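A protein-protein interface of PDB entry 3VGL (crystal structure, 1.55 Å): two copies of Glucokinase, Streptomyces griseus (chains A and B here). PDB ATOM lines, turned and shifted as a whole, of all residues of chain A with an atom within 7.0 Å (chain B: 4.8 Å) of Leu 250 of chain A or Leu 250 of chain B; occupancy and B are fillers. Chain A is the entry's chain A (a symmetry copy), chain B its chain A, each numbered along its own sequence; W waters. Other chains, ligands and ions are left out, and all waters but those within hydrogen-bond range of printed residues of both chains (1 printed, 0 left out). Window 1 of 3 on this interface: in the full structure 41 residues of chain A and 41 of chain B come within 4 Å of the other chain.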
ATOM      1  N   ILE A 138      32.314  19.483  -8.159  1.00  0.00           N
ATOM      2  CA  ILE A 138      31.376  20.278  -8.959  1.00  0.00           C
ATOM      3  C   ILE A 138      31.109  21.609  -8.266  1.00  0.00           C
ATOM      4  O   ILE A 138      30.633  21.649  -7.130  1.00  0.00           O
ATOM      5  CB  ILE A 138      30.024  19.545  -9.097  1.00  0.00           C
ATOM      6  CG1 ILE A 138      30.174  18.221  -9.835  1.00  0.00           C
ATOM      7  CG2 ILE A 138      28.983  20.425  -9.849  1.00  0.00           C
ATOM      8  CD1 ILE A 138      29.017  17.312  -9.588  1.00  0.00           C
ATOM      9  N   ARG A 145      28.527  21.290  -5.136  1.00  0.00           N
ATOM     10  CA  ARG A 145      27.349  20.445  -5.256  1.00  0.00           C
ATOM     11  C   ARG A 145      27.664  18.988  -4.941  1.00  0.00           C
ATOM     12  O   ARG A 145      28.374  18.313  -5.690  1.00  0.00           O
ATOM     13  CB  ARG A 145      26.741  20.540  -6.657  1.00  0.00           C
ATOM     14  CG  ARG A 145      26.475  21.961  -7.141  1.00  0.00           C
ATOM     15  CD  ARG A 145      25.406  22.661  -6.307  1.00  0.00           C
ATOM     16  NE  ARG A 145      25.243  24.037  -6.757  1.00  0.00           N
ATOM     17  CZ  ARG A 145      24.226  24.823  -6.408  1.00  0.00           C
ATOM     18  NH1 ARG A 145      23.254  24.367  -5.631  1.00  0.00           N
ATOM     19  NH2 ARG A 145      24.171  26.067  -6.862  1.00  0.00           N
ATOM     20  N   VAL A 151      26.950  12.050  -2.605  1.00  0.00           N
ATOM     21  CA  VAL A 151      27.912  11.298  -3.414  1.00  0.00           C
ATOM     22  C   VAL A 151      27.949  11.654  -4.901  1.00  0.00           C
ATOM     23  O   VAL A 151      28.390  10.837  -5.737  1.00  0.00           O
ATOM     24  CB  VAL A 151      27.774   9.779  -3.198  1.00  0.00           C
ATOM     25  CG1 VAL A 151      28.011   9.427  -1.715  1.00  0.00           C
ATOM     26  CG2 VAL A 151      26.407   9.263  -3.677  1.00  0.00           C
ATOM     27  N   ALA A 152      27.575  12.892  -5.223  1.00  0.00           N
ATOM     28  CA  ALA A 152      27.825  13.426  -6.567  1.00  0.00           C
ATOM     29  C   ALA A 152      29.324  13.491  -6.854  1.00  0.00           C
ATOM     30  O   ALA A 152      30.164  13.381  -5.934  1.00  0.00           O
ATOM     31  CB  ALA A 152      27.183  14.813  -6.746  1.00  0.00           C
ATOM     32  N   ALA A 153      29.648  13.672  -8.130  1.00  0.00           N
ATOM     33  CA  ALA A 153      31.024  13.939  -8.564  1.00  0.00           C
ATOM     34  C   ALA A 153      31.953  12.747  -8.329  1.00  0.00           C
ATOM     35  O   ALA A 153      33.164  12.907  -8.146  1.00  0.00           O
ATOM     36  CB  ALA A 153      31.578  15.215  -7.910  1.00  0.00           C
ATOM     37  N   GLU A 154      31.395  11.549  -8.405  1.00  0.00           N
ATOM     38  CA  GLU A 154      32.212  10.339  -8.400  1.00  0.00           C
ATOM     39  C   GLU A 154      32.587   9.971  -9.839  1.00  0.00           C
ATOM     40  O   GLU A 154      32.270   8.880 -10.347  1.00  0.00           O
ATOM     41  CB  GLU A 154      31.478   9.223  -7.663  1.00  0.00           C
ATOM     42  CG  GLU A 154      31.635   9.380  -6.135  1.00  0.00           C
ATOM     43  CD  GLU A 154      33.090   9.304  -5.731  1.00  0.00           C
ATOM     44  OE1 GLU A 154      33.793   8.428  -6.301  1.00  0.00           O
ATOM     45  OE2 GLU A 154      33.496  10.118  -4.858  1.00  0.00           O
ATOM     46  N   PHE A 155      33.282  10.908 -10.486  1.00  0.00           N
ATOM     47  CA  PHE A 155      33.576  10.774 -11.910  1.00  0.00           C
ATOM     48  C   PHE A 155      34.468   9.563 -12.218  1.00  0.00           C
ATOM     49  O   PHE A 155      34.451   9.015 -13.339  1.00  0.00           O
ATOM     50  CB  PHE A 155      34.356  11.996 -12.419  1.00  0.00           C
ATOM     51  CG  PHE A 155      33.659  13.323 -12.240  1.00  0.00           C
ATOM     52  CD1 PHE A 155      32.272  13.427 -12.104  1.00  0.00           C
ATOM     53  CD2 PHE A 155      34.422  14.486 -12.291  1.00  0.00           C
ATOM     54  CE1 PHE A 155      31.661  14.698 -11.971  1.00  0.00           C
ATOM     55  CE2 PHE A 155      33.838  15.736 -12.155  1.00  0.00           C
ATOM     56  CZ  PHE A 155      32.462  15.853 -11.988  1.00  0.00           C
ATOM     57  N   ILE A 158      32.507   6.487 -13.595  1.00  0.00           N
ATOM     58  CA  ILE A 158      31.748   6.512 -14.856  1.00  0.00           C
ATOM     59  C   ILE A 158      32.360   5.440 -15.753  1.00  0.00           C
ATOM     60  O   ILE A 158      33.577   5.296 -15.819  1.00  0.00           O
ATOM     61  CB  ILE A 158      31.917   7.889 -15.559  1.00  0.00           C
ATOM     62  CG1 ILE A 158      31.232   8.978 -14.716  1.00  0.00           C
ATOM     63  CG2 ILE A 158      31.358   7.861 -16.997  1.00  0.00           C
ATOM     64  CD1 ILE A 158      31.776  10.367 -15.101  1.00  0.00           C
ATOM     65  N   TRP A 175      36.356   5.052 -15.467  1.00  0.00           N
ATOM     66  CA  TRP A 175      37.304   6.059 -15.926  1.00  0.00           C
ATOM     67  C   TRP A 175      38.634   6.041 -15.145  1.00  0.00           C
ATOM     68  O   TRP A 175      39.704   6.160 -15.729  1.00  0.00           O
ATOM     69  CB  TRP A 175      36.636   7.448 -15.880  1.00  0.00           C
ATOM     70  CG  TRP A 175      37.404   8.546 -16.579  1.00  0.00           C
ATOM     71  CD1 TRP A 175      38.364   8.415 -17.567  1.00  0.00           C
ATOM     72  CD2 TRP A 175      37.178   9.936 -16.414  1.00  0.00           C
ATOM     73  NE1 TRP A 175      38.787   9.666 -17.971  1.00  0.00           N
ATOM     74  CE2 TRP A 175      38.059  10.612 -17.289  1.00  0.00           C
ATOM     75  CE3 TRP A 175      36.315  10.681 -15.596  1.00  0.00           C
ATOM     76  CZ2 TRP A 175      38.121  12.016 -17.358  1.00  0.00           C
ATOM     77  CZ3 TRP A 175      36.358  12.079 -15.677  1.00  0.00           C
ATOM     78  CH2 TRP A 175      37.268  12.725 -16.547  1.00  0.00           C
ATOM     79  N   GLY A 243      37.524  12.029 -21.442  1.00  0.00           N
ATOM     80  CA  GLY A 243      36.593  12.156 -20.332  1.00  0.00           C
ATOM     81  C   GLY A 243      36.217  13.600 -20.063  1.00  0.00           C
ATOM     82  O   GLY A 243      35.076  13.883 -19.722  1.00  0.00           O
ATOM     83  N   LEU A 244      37.184  14.523 -20.142  1.00  0.00           N
ATOM     84  CA  LEU A 244      36.861  15.952 -20.001  1.00  0.00           C
ATOM     85  C   LEU A 244      35.896  16.412 -21.083  1.00  0.00           C
ATOM     86  O   LEU A 244      35.000  17.235 -20.816  1.00  0.00           O
ATOM     87  CB  LEU A 244      38.121  16.830 -20.056  1.00  0.00           C
ATOM     88  CG  LEU A 244      39.036  16.776 -18.830  1.00  0.00           C
ATOM     89  CD1 LEU A 244      40.183  17.736 -19.065  1.00  0.00           C
ATOM     90  CD2 LEU A 244      38.326  17.110 -17.515  1.00  0.00           C
ATOM     91  N   ALA A 245      36.065  15.885 -22.298  1.00  0.00           N
ATOM     92  CA  ALA A 245      35.086  16.215 -23.352  1.00  0.00           C
ATOM     93  C   ALA A 245      33.697  15.712 -22.972  1.00  0.00           C
ATOM     94  O   ALA A 245      32.696  16.441 -23.159  1.00  0.00           O
ATOM     95  CB  ALA A 245      35.539  15.700 -24.681  1.00  0.00           C
ATOM     96  N   ASP A 246      33.607  14.506 -22.416  1.00  0.00           N
ATOM     97  CA  ASP A 246      32.294  14.030 -21.895  1.00  0.00           C
ATOM     98  C   ASP A 246      31.750  14.934 -20.763  1.00  0.00           C
ATOM     99  O   ASP A 246      30.547  15.240 -20.694  1.00  0.00           O
ATOM    100  CB  ASP A 246      32.375  12.578 -21.404  1.00  0.00           C
ATOM    101  CG  ASP A 246      32.509  11.556 -22.555  1.00  0.00           C
ATOM    102  OD1 ASP A 246      32.227  11.876 -23.718  1.00  0.00           O
ATOM    103  OD2 ASP A 246      32.943  10.428 -22.257  1.00  0.00           O
ATOM    104  N   LEU A 247      32.635  15.387 -19.878  1.00  0.00           N
ATOM    105  CA  LEU A 247      32.181  16.291 -18.826  1.00  0.00           C
ATOM    106  C   LEU A 247      31.704  17.631 -19.381  1.00  0.00           C
ATOM    107  O   LEU A 247      30.860  18.281 -18.734  1.00  0.00           O
ATOM    108  CB  LEU A 247      33.285  16.509 -17.788  1.00  0.00           C
ATOM    109  CG  LEU A 247      33.710  15.291 -16.959  1.00  0.00           C
ATOM    110  CD1 LEU A 247      34.843  15.677 -15.994  1.00  0.00           C
ATOM    111  CD2 LEU A 247      32.566  14.758 -16.115  1.00  0.00           C
ATOM    112  N   ALA A 248      32.252  18.060 -20.525  1.00  0.00           N
ATOM    113  CA  ALA A 248      31.772  19.291 -21.191  1.00  0.00           C
ATOM    114  C   ALA A 248      30.355  19.059 -21.699  1.00  0.00           C
ATOM    115  O   ALA A 248      29.507  19.975 -21.612  1.00  0.00           O
ATOM    116  CB  ALA A 248      32.697  19.707 -22.336  1.00  0.00           C
ATOM    117  N   SER A 249      30.108  17.853 -22.235  1.00  0.00           N
ATOM    118  CA  SER A 249      28.735  17.487 -22.670  1.00  0.00           C
ATOM    119  C   SER A 249      27.768  17.505 -21.503  1.00  0.00           C
ATOM    120  O   SER A 249      26.625  17.956 -21.656  1.00  0.00           O
ATOM    121  CB  SER A 249      28.725  16.127 -23.350  1.00  0.00           C
ATOM    122  OG  SER A 249      29.423  16.265 -24.557  1.00  0.00           O
ATOM    123  N   LEU A 250      28.236  17.062 -20.339  1.00  0.00           N
ATOM    124  CA  LEU A 250      27.413  16.962 -19.130  1.00  0.00           C
ATOM    125  C   LEU A 250      27.167  18.322 -18.477  1.00  0.00           C
ATOM    126  O   LEU A 250      26.000  18.701 -18.240  1.00  0.00           O
ATOM    127  CB  LEU A 250      28.056  16.000 -18.138  1.00  0.00           C
ATOM    128  CG  LEU A 250      27.936  14.542 -18.576  1.00  0.00           C
ATOM    129  CD1 LEU A 250      29.176  13.739 -18.194  1.00  0.00           C
ATOM    130  CD2 LEU A 250      26.697  13.935 -17.912  1.00  0.00           C
ATOM    131  N   PHE A 251      28.248  19.060 -18.200  1.00  0.00           N
ATOM    132  CA  PHE A 251      28.193  20.251 -17.325  1.00  0.00           C
ATOM    133  C   PHE A 251      28.401  21.577 -18.045  1.00  0.00           C
ATOM    134  O   PHE A 251      28.000  22.634 -17.533  1.00  0.00           O
ATOM    135  CB  PHE A 251      29.271  20.153 -16.233  1.00  0.00           C
ATOM    136  CG  PHE A 251      29.038  19.064 -15.230  1.00  0.00           C
ATOM    137  CD1 PHE A 251      28.107  19.236 -14.203  1.00  0.00           C
ATOM    138  CD2 PHE A 251      29.791  17.886 -15.274  1.00  0.00           C
ATOM    139  CE1 PHE A 251      27.902  18.212 -13.251  1.00  0.00           C
ATOM    140  CE2 PHE A 251      29.574  16.866 -14.331  1.00  0.00           C
ATOM    141  CZ  PHE A 251      28.642  17.048 -13.312  1.00  0.00           C
ATOM    142  N   ASP A 252      29.049  21.536 -19.210  1.00  0.00           N
ATOM    143  CA  ASP A 252      29.428  22.783 -19.933  1.00  0.00           C
ATOM    144  C   ASP A 252      29.968  23.914 -19.021  1.00  0.00           C
ATOM    145  O   ASP A 252      29.403  25.024 -19.002  1.00  0.00           O
ATOM    146  CB  ASP A 252      28.232  23.282 -20.774  1.00  0.00           C
ATOM    147  CG  ASP A 252      28.586  24.461 -21.684  1.00  0.00           C
ATOM    148  OD1 ASP A 252      29.698  24.464 -22.258  1.00  0.00           O
ATOM    149  OD2 ASP A 252      27.725  25.356 -21.863  1.00  0.00           O
ATOM    150  N   PRO A 253      31.053  23.656 -18.258  1.00  0.00           N
ATOM    151  CA  PRO A 253      31.590  24.683 -17.343  1.00  0.00           C
ATOM    152  C   PRO A 253      32.449  25.692 -18.110  1.00  0.00           C
ATOM    153  O   PRO A 253      32.781  25.463 -19.272  1.00  0.00           O
ATOM    154  CB  PRO A 253      32.469  23.865 -16.407  1.00  0.00           C
ATOM    155  CG  PRO A 253      33.049  22.829 -17.340  1.00  0.00           C
ATOM    156  CD  PRO A 253      31.886  22.428 -18.239  1.00  0.00           C
ATOM    157  N   ILE B 138      18.988  19.330 -16.581  1.00  0.00           N
ATOM    158  CA  ILE B 138      19.572  19.355 -15.236  1.00  0.00           C
ATOM    159  C   ILE B 138      18.827  20.366 -14.371  1.00  0.00           C
ATOM    160  O   ILE B 138      18.773  21.555 -14.689  1.00  0.00           O
ATOM    161  CB  ILE B 138      21.051  19.793 -15.294  1.00  0.00           C
ATOM    162  CG1 ILE B 138      21.898  18.809 -16.091  1.00  0.00           C
ATOM    163  CG2 ILE B 138      21.653  19.930 -13.865  1.00  0.00           C
ATOM    164  CD1 ILE B 138      23.185  19.417 -16.538  1.00  0.00           C
ATOM    165  N   ALA B 152      25.100  22.742 -21.632  1.00  0.00           N
ATOM    166  CA  ALA B 152      25.098  21.633 -20.671  1.00  0.00           C
ATOM    167  C   ALA B 152      24.010  20.619 -21.016  1.00  0.00           C
ATOM    168  O   ALA B 152      23.096  20.900 -21.823  1.00  0.00           O
ATOM    169  CB  ALA B 152      24.921  22.142 -19.231  1.00  0.00           C
ATOM    170  N   ALA B 153      24.115  19.446 -20.400  1.00  0.00           N
ATOM    171  CA  ALA B 153      23.065  18.422 -20.469  1.00  0.00           C
ATOM    172  C   ALA B 153      22.898  17.850 -21.878  1.00  0.00           C
ATOM    173  O   ALA B 153      21.815  17.394 -22.258  1.00  0.00           O
ATOM    174  CB  ALA B 153      21.731  18.953 -19.921  1.00  0.00           C
ATOM    175  N   PHE B 155      23.609  14.966 -22.864  1.00  0.00           N
ATOM    176  CA  PHE B 155      23.956  13.616 -22.426  1.00  0.00           C
ATOM    177  C   PHE B 155      24.019  12.616 -23.590  1.00  0.00           C
ATOM    178  O   PHE B 155      24.719  11.585 -23.520  1.00  0.00           O
ATOM    179  CB  PHE B 155      22.886  13.065 -21.472  1.00  0.00           C
ATOM    180  CG  PHE B 155      22.657  13.883 -20.223  1.00  0.00           C
ATOM    181  CD1 PHE B 155      23.624  14.752 -19.712  1.00  0.00           C
ATOM    182  CD2 PHE B 155      21.470  13.701 -19.520  1.00  0.00           C
ATOM    183  CE1 PHE B 155      23.373  15.475 -18.518  1.00  0.00           C
ATOM    184  CE2 PHE B 155      21.209  14.406 -18.354  1.00  0.00           C
ATOM    185  CZ  PHE B 155      22.150  15.299 -17.850  1.00  0.00           C
ATOM    186  N   ILE B 158      27.647  11.831 -24.782  1.00  0.00           N
ATOM    187  CA  ILE B 158      28.665  11.210 -23.918  1.00  0.00           C
ATOM    188  C   ILE B 158      29.078   9.908 -24.600  1.00  0.00           C
ATOM    189  O   ILE B 158      28.239   9.177 -25.117  1.00  0.00           O
ATOM    190  CB  ILE B 158      28.052  10.859 -22.532  1.00  0.00           C
ATOM    191  CG1 ILE B 158      27.706  12.159 -21.786  1.00  0.00           C
ATOM    192  CG2 ILE B 158      29.005   9.975 -21.701  1.00  0.00           C
ATOM    193  CD1 ILE B 158      26.685  11.872 -20.667  1.00  0.00           C
ATOM    194  N   ASP B 246      25.660   5.868 -14.593  1.00  0.00           N
ATOM    195  CA  ASP B 246      26.741   6.882 -14.757  1.00  0.00           C
ATOM    196  C   ASP B 246      26.281   8.300 -14.343  1.00  0.00           C
ATOM    197  O   ASP B 246      27.022   9.064 -13.701  1.00  0.00           O
ATOM    198  CB  ASP B 246      27.275   6.909 -16.195  1.00  0.00           C
ATOM    199  CG  ASP B 246      28.120   5.666 -16.551  1.00  0.00           C
ATOM    200  OD1 ASP B 246      28.577   4.938 -15.660  1.00  0.00           O
ATOM    201  OD2 ASP B 246      28.278   5.422 -17.762  1.00  0.00           O
ATOM    202  N   LEU B 247      25.046   8.657 -14.690  1.00  0.00           N
ATOM    203  CA  LEU B 247      24.546   9.963 -14.272  1.00  0.00           C
ATOM    204  C   LEU B 247      24.399  10.067 -12.755  1.00  0.00           C
ATOM    205  O   LEU B 247      24.477  11.191 -12.222  1.00  0.00           O
ATOM    206  CB  LEU B 247      23.214  10.274 -14.957  1.00  0.00           C
ATOM    207  CG  LEU B 247      23.239  10.449 -16.480  1.00  0.00           C
ATOM    208  CD1 LEU B 247      21.820  10.725 -17.004  1.00  0.00           C
ATOM    209  CD2 LEU B 247      24.106  11.624 -16.897  1.00  0.00           C
ATOM    210  N   ALA B 248      24.153   8.939 -12.076  1.00  0.00           N
ATOM    211  CA  ALA B 248      24.105   8.931 -10.597  1.00  0.00           C
ATOM    212  C   ALA B 248      25.500   9.214 -10.054  1.00  0.00           C
ATOM    213  O   ALA B 248      25.638   9.943  -9.046  1.00  0.00           O
ATOM    214  CB  ALA B 248      23.575   7.599 -10.060  1.00  0.00           C
ATOM    215  N   SER B 249      26.519   8.633 -10.707  1.00  0.00           N
ATOM    216  CA  SER B 249      27.925   8.922 -10.324  1.00  0.00           C
ATOM    217  C   SER B 249      28.249  10.392 -10.501  1.00  0.00           C
ATOM    218  O   SER B 249      28.945  10.975  -9.659  1.00  0.00           O
ATOM    219  CB  SER B 249      28.894   8.063 -11.120  1.00  0.00           C
ATOM    220  OG  SER B 249      28.708   6.738 -10.703  1.00  0.00           O
ATOM    221  N   LEU B 250      27.713  10.994 -11.559  1.00  0.00           N
ATOM    222  CA  LEU B 250      27.974  12.395 -11.902  1.00  0.00           C
ATOM    223  C   LEU B 250      27.212  13.368 -11.003  1.00  0.00           C
ATOM    224  O   LEU B 250      27.827  14.266 -10.390  1.00  0.00           O
ATOM    225  CB  LEU B 250      27.638  12.646 -13.367  1.00  0.00           C
ATOM    226  CG  LEU B 250      28.658  12.020 -14.316  1.00  0.00           C
ATOM    227  CD1 LEU B 250      27.994  11.492 -15.584  1.00  0.00           C
ATOM    228  CD2 LEU B 250      29.701  13.081 -14.678  1.00  0.00           C
ATOM    229  N   PHE B 251      25.889  13.190 -10.908  1.00  0.00           N
ATOM    230  CA  PHE B 251      24.991  14.205 -10.315  1.00  0.00           C
ATOM    231  C   PHE B 251      24.382  13.808  -8.977  1.00  0.00           C
ATOM    232  O   PHE B 251      23.950  14.679  -8.206  1.00  0.00           O
ATOM    233  CB  PHE B 251      23.827  14.502 -11.274  1.00  0.00           C
ATOM    234  CG  PHE B 251      24.230  15.197 -12.539  1.00  0.00           C
ATOM    235  CD1 PHE B 251      24.495  16.569 -12.539  1.00  0.00           C
ATOM    236  CD2 PHE B 251      24.290  14.494 -13.747  1.00  0.00           C
ATOM    237  CE1 PHE B 251      24.859  17.221 -13.738  1.00  0.00           C
ATOM    238  CE2 PHE B 251      24.665  15.147 -14.934  1.00  0.00           C
ATOM    239  CZ  PHE B 251      24.928  16.515 -14.922  1.00  0.00           C
ATOM    240  N   ASP B 252      24.316  12.503  -8.707  1.00  0.00           N
ATOM    241  CA  ASP B 252      23.617  11.994  -7.492  1.00  0.00           C
ATOM    242  C   ASP B 252      22.279  12.711  -7.176  1.00  0.00           C
ATOM    243  O   ASP B 252      22.120  13.279  -6.079  1.00  0.00           O
ATOM    244  CB  ASP B 252      24.572  12.056  -6.279  1.00  0.00           C
ATOM    245  CG  ASP B 252      23.994  11.393  -5.025  1.00  0.00           C
ATOM    246  OD1 ASP B 252      23.338  10.335  -5.153  1.00  0.00           O
ATOM    247  OD2 ASP B 252      24.247  11.907  -3.908  1.00  0.00           O
HETATM  248  O   HOH W   1      27.388   8.855  -7.197  1.00  0.00           O
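N of Ala 153 of chain B is in hydrogen-bond range of O of Ser 249 of chain A (3.2 Å).
N of Ala 153 of chain B is in hydrogen-bond range of O of Leu 250 of chain A, 3.0 Å away.
The backbone NH (N) of Ala 153 of chain A lies within hydrogen-bond range of the backbone carbonyl oxygen (O) of Ser 249 of chain B (3.2 Å).
The backbone carbonyl oxygen (O) of Ser 249 of chain B is in hydrogen-bond range of the backbone NH (N) of Glu 154 of chain A, 2.8 Å away.
O of Leu 250 of chain B sits at hydrogen-bond distance from N of Ala 153 of chain A (3.0 Å).
OD2 of Asp 252 of chain B sits at hydrogen-bond distance from N of Val 151 of chain A, 3.0 Å away.
Among the printed residues, pairs that only touch across the chains: Ile 138 of chain A with Leu 250 of chain B, Val 151 of chain A with Ser 249 of chain B, Ala 152 of chain A with Ser 249 of chain B, Ala 152 of chain A with Leu 250 of chain B, Ala 152 of chain A with Phe 251 of chain B, Ala 152 of chain A with Asp 252 of chain B, Phe 155 of chain A with Leu 250 of chain B, Ile 158 of chain A with Asp 246 of chain B, Ile 158 of chain A with Leu 250 of chain B, Asp 246 of chain A with Ile 158 of chain B, Leu 247 of chain A with Leu 250 of chain B, Ser 249 of chain A with Ala 152 of chain B, Leu 250 of chain A with Ile 138 of chain B, Leu 250 of chain A with Ala 152 of chain B, Leu 250 of chain A with Phe 155 of chain B, Leu 250 of chain A with Ile 158 of chain B, Leu 250 of chain A with Leu 247 of chain B, Leu 250 of chain A with Leu 250 of chain B, Leu 250 of chain A with Phe 251 of chain B, Phe 251 of chain A with Ala 152 of chain B, Phe 251 of chain A with Leu 250 of chain B, Phe 251 of chain A with Phe 251 of chain B and Asp 252 of chain A with Ala 152 of chain B.
Ile 138 of chain A touches Leu 250 of chain B, and with the chains exchanged Leu 250 of chain A touches Ile 138 of chain B.
Ala 153 of chain A touches Leu 250 of chain B, and with the chains exchanged Leu 250 of chain A touches Ala 153 of chain B.
Phe 155 of chain A touches Leu 250 of chain B, and with the chains exchanged Leu 250 of chain A touches Phe 155 of chain B.
Ile 158 of chain A touches Asp 246 of chain B, and with the chains exchanged Asp 246 of chain A touches Ile 158 of chain B.
Positions printed for both chains: 138, 152, 153, 155, 158, 246, 247, 248, 249, 250, 251 and 252.
Of the 29 pairs that touch across the chains among the printed residues, 26 have their exchanged pair printed and touching as well.
Of the printed residues of chain B, Ile 158 of chain A touches Asp 246 (3.6 Å) and Leu 250 (3.4 Å).
Printed residues of chain B within 4 Å of Ser 249 of chain A: Ala 152 (3.8 Å) and Ala 153 (3.2 Å).
Leu 250 of chain A touches eight residues of chain B.
Pro 253 of chain A touches none of the printed residues of chain B.
Ala 248 of chain B touches none of the printed residues of chain A.
Leu 250 of chain B touches eight residues of chain A.
The nearest printed residue of chain B that does not touch Leu 250 of chain A is Asp 246 of chain B (6.4 Å).
Of the 12 printed residues of chain B, 11 touch a printed residue of chain A.
Printed residues of chain B that touch a printed residue of chain A: Ile 138, Ala 152, Ala 153, Phe 155, Ile 158, Asp 246, Leu 247, Ser 249, Leu 250, Phe 251 and Asp 252.
Along chain A the printed residues that touch a printed residue of chain B span positions 138 to 252.
Among the printed residues, no Asp or Glu carboxylate lies within 4 Å of a Lys or Arg side-chain nitrogen of the other chain.
Water W1 lies within hydrogen-bond range of O of Val 151 of chain A (2.7 Å) and O of Ala 248 of chain B (2.8 Å).
The backbone NH of Arg 145 of chain A lies within hydrogen-bond range of the backbone carbonyl oxygen of Ile 138 of chain A (2.9 Å).
O of Ile 158 of chain A sits at hydrogen-bond distance from N of Trp 175 of chain A (2.8 Å).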
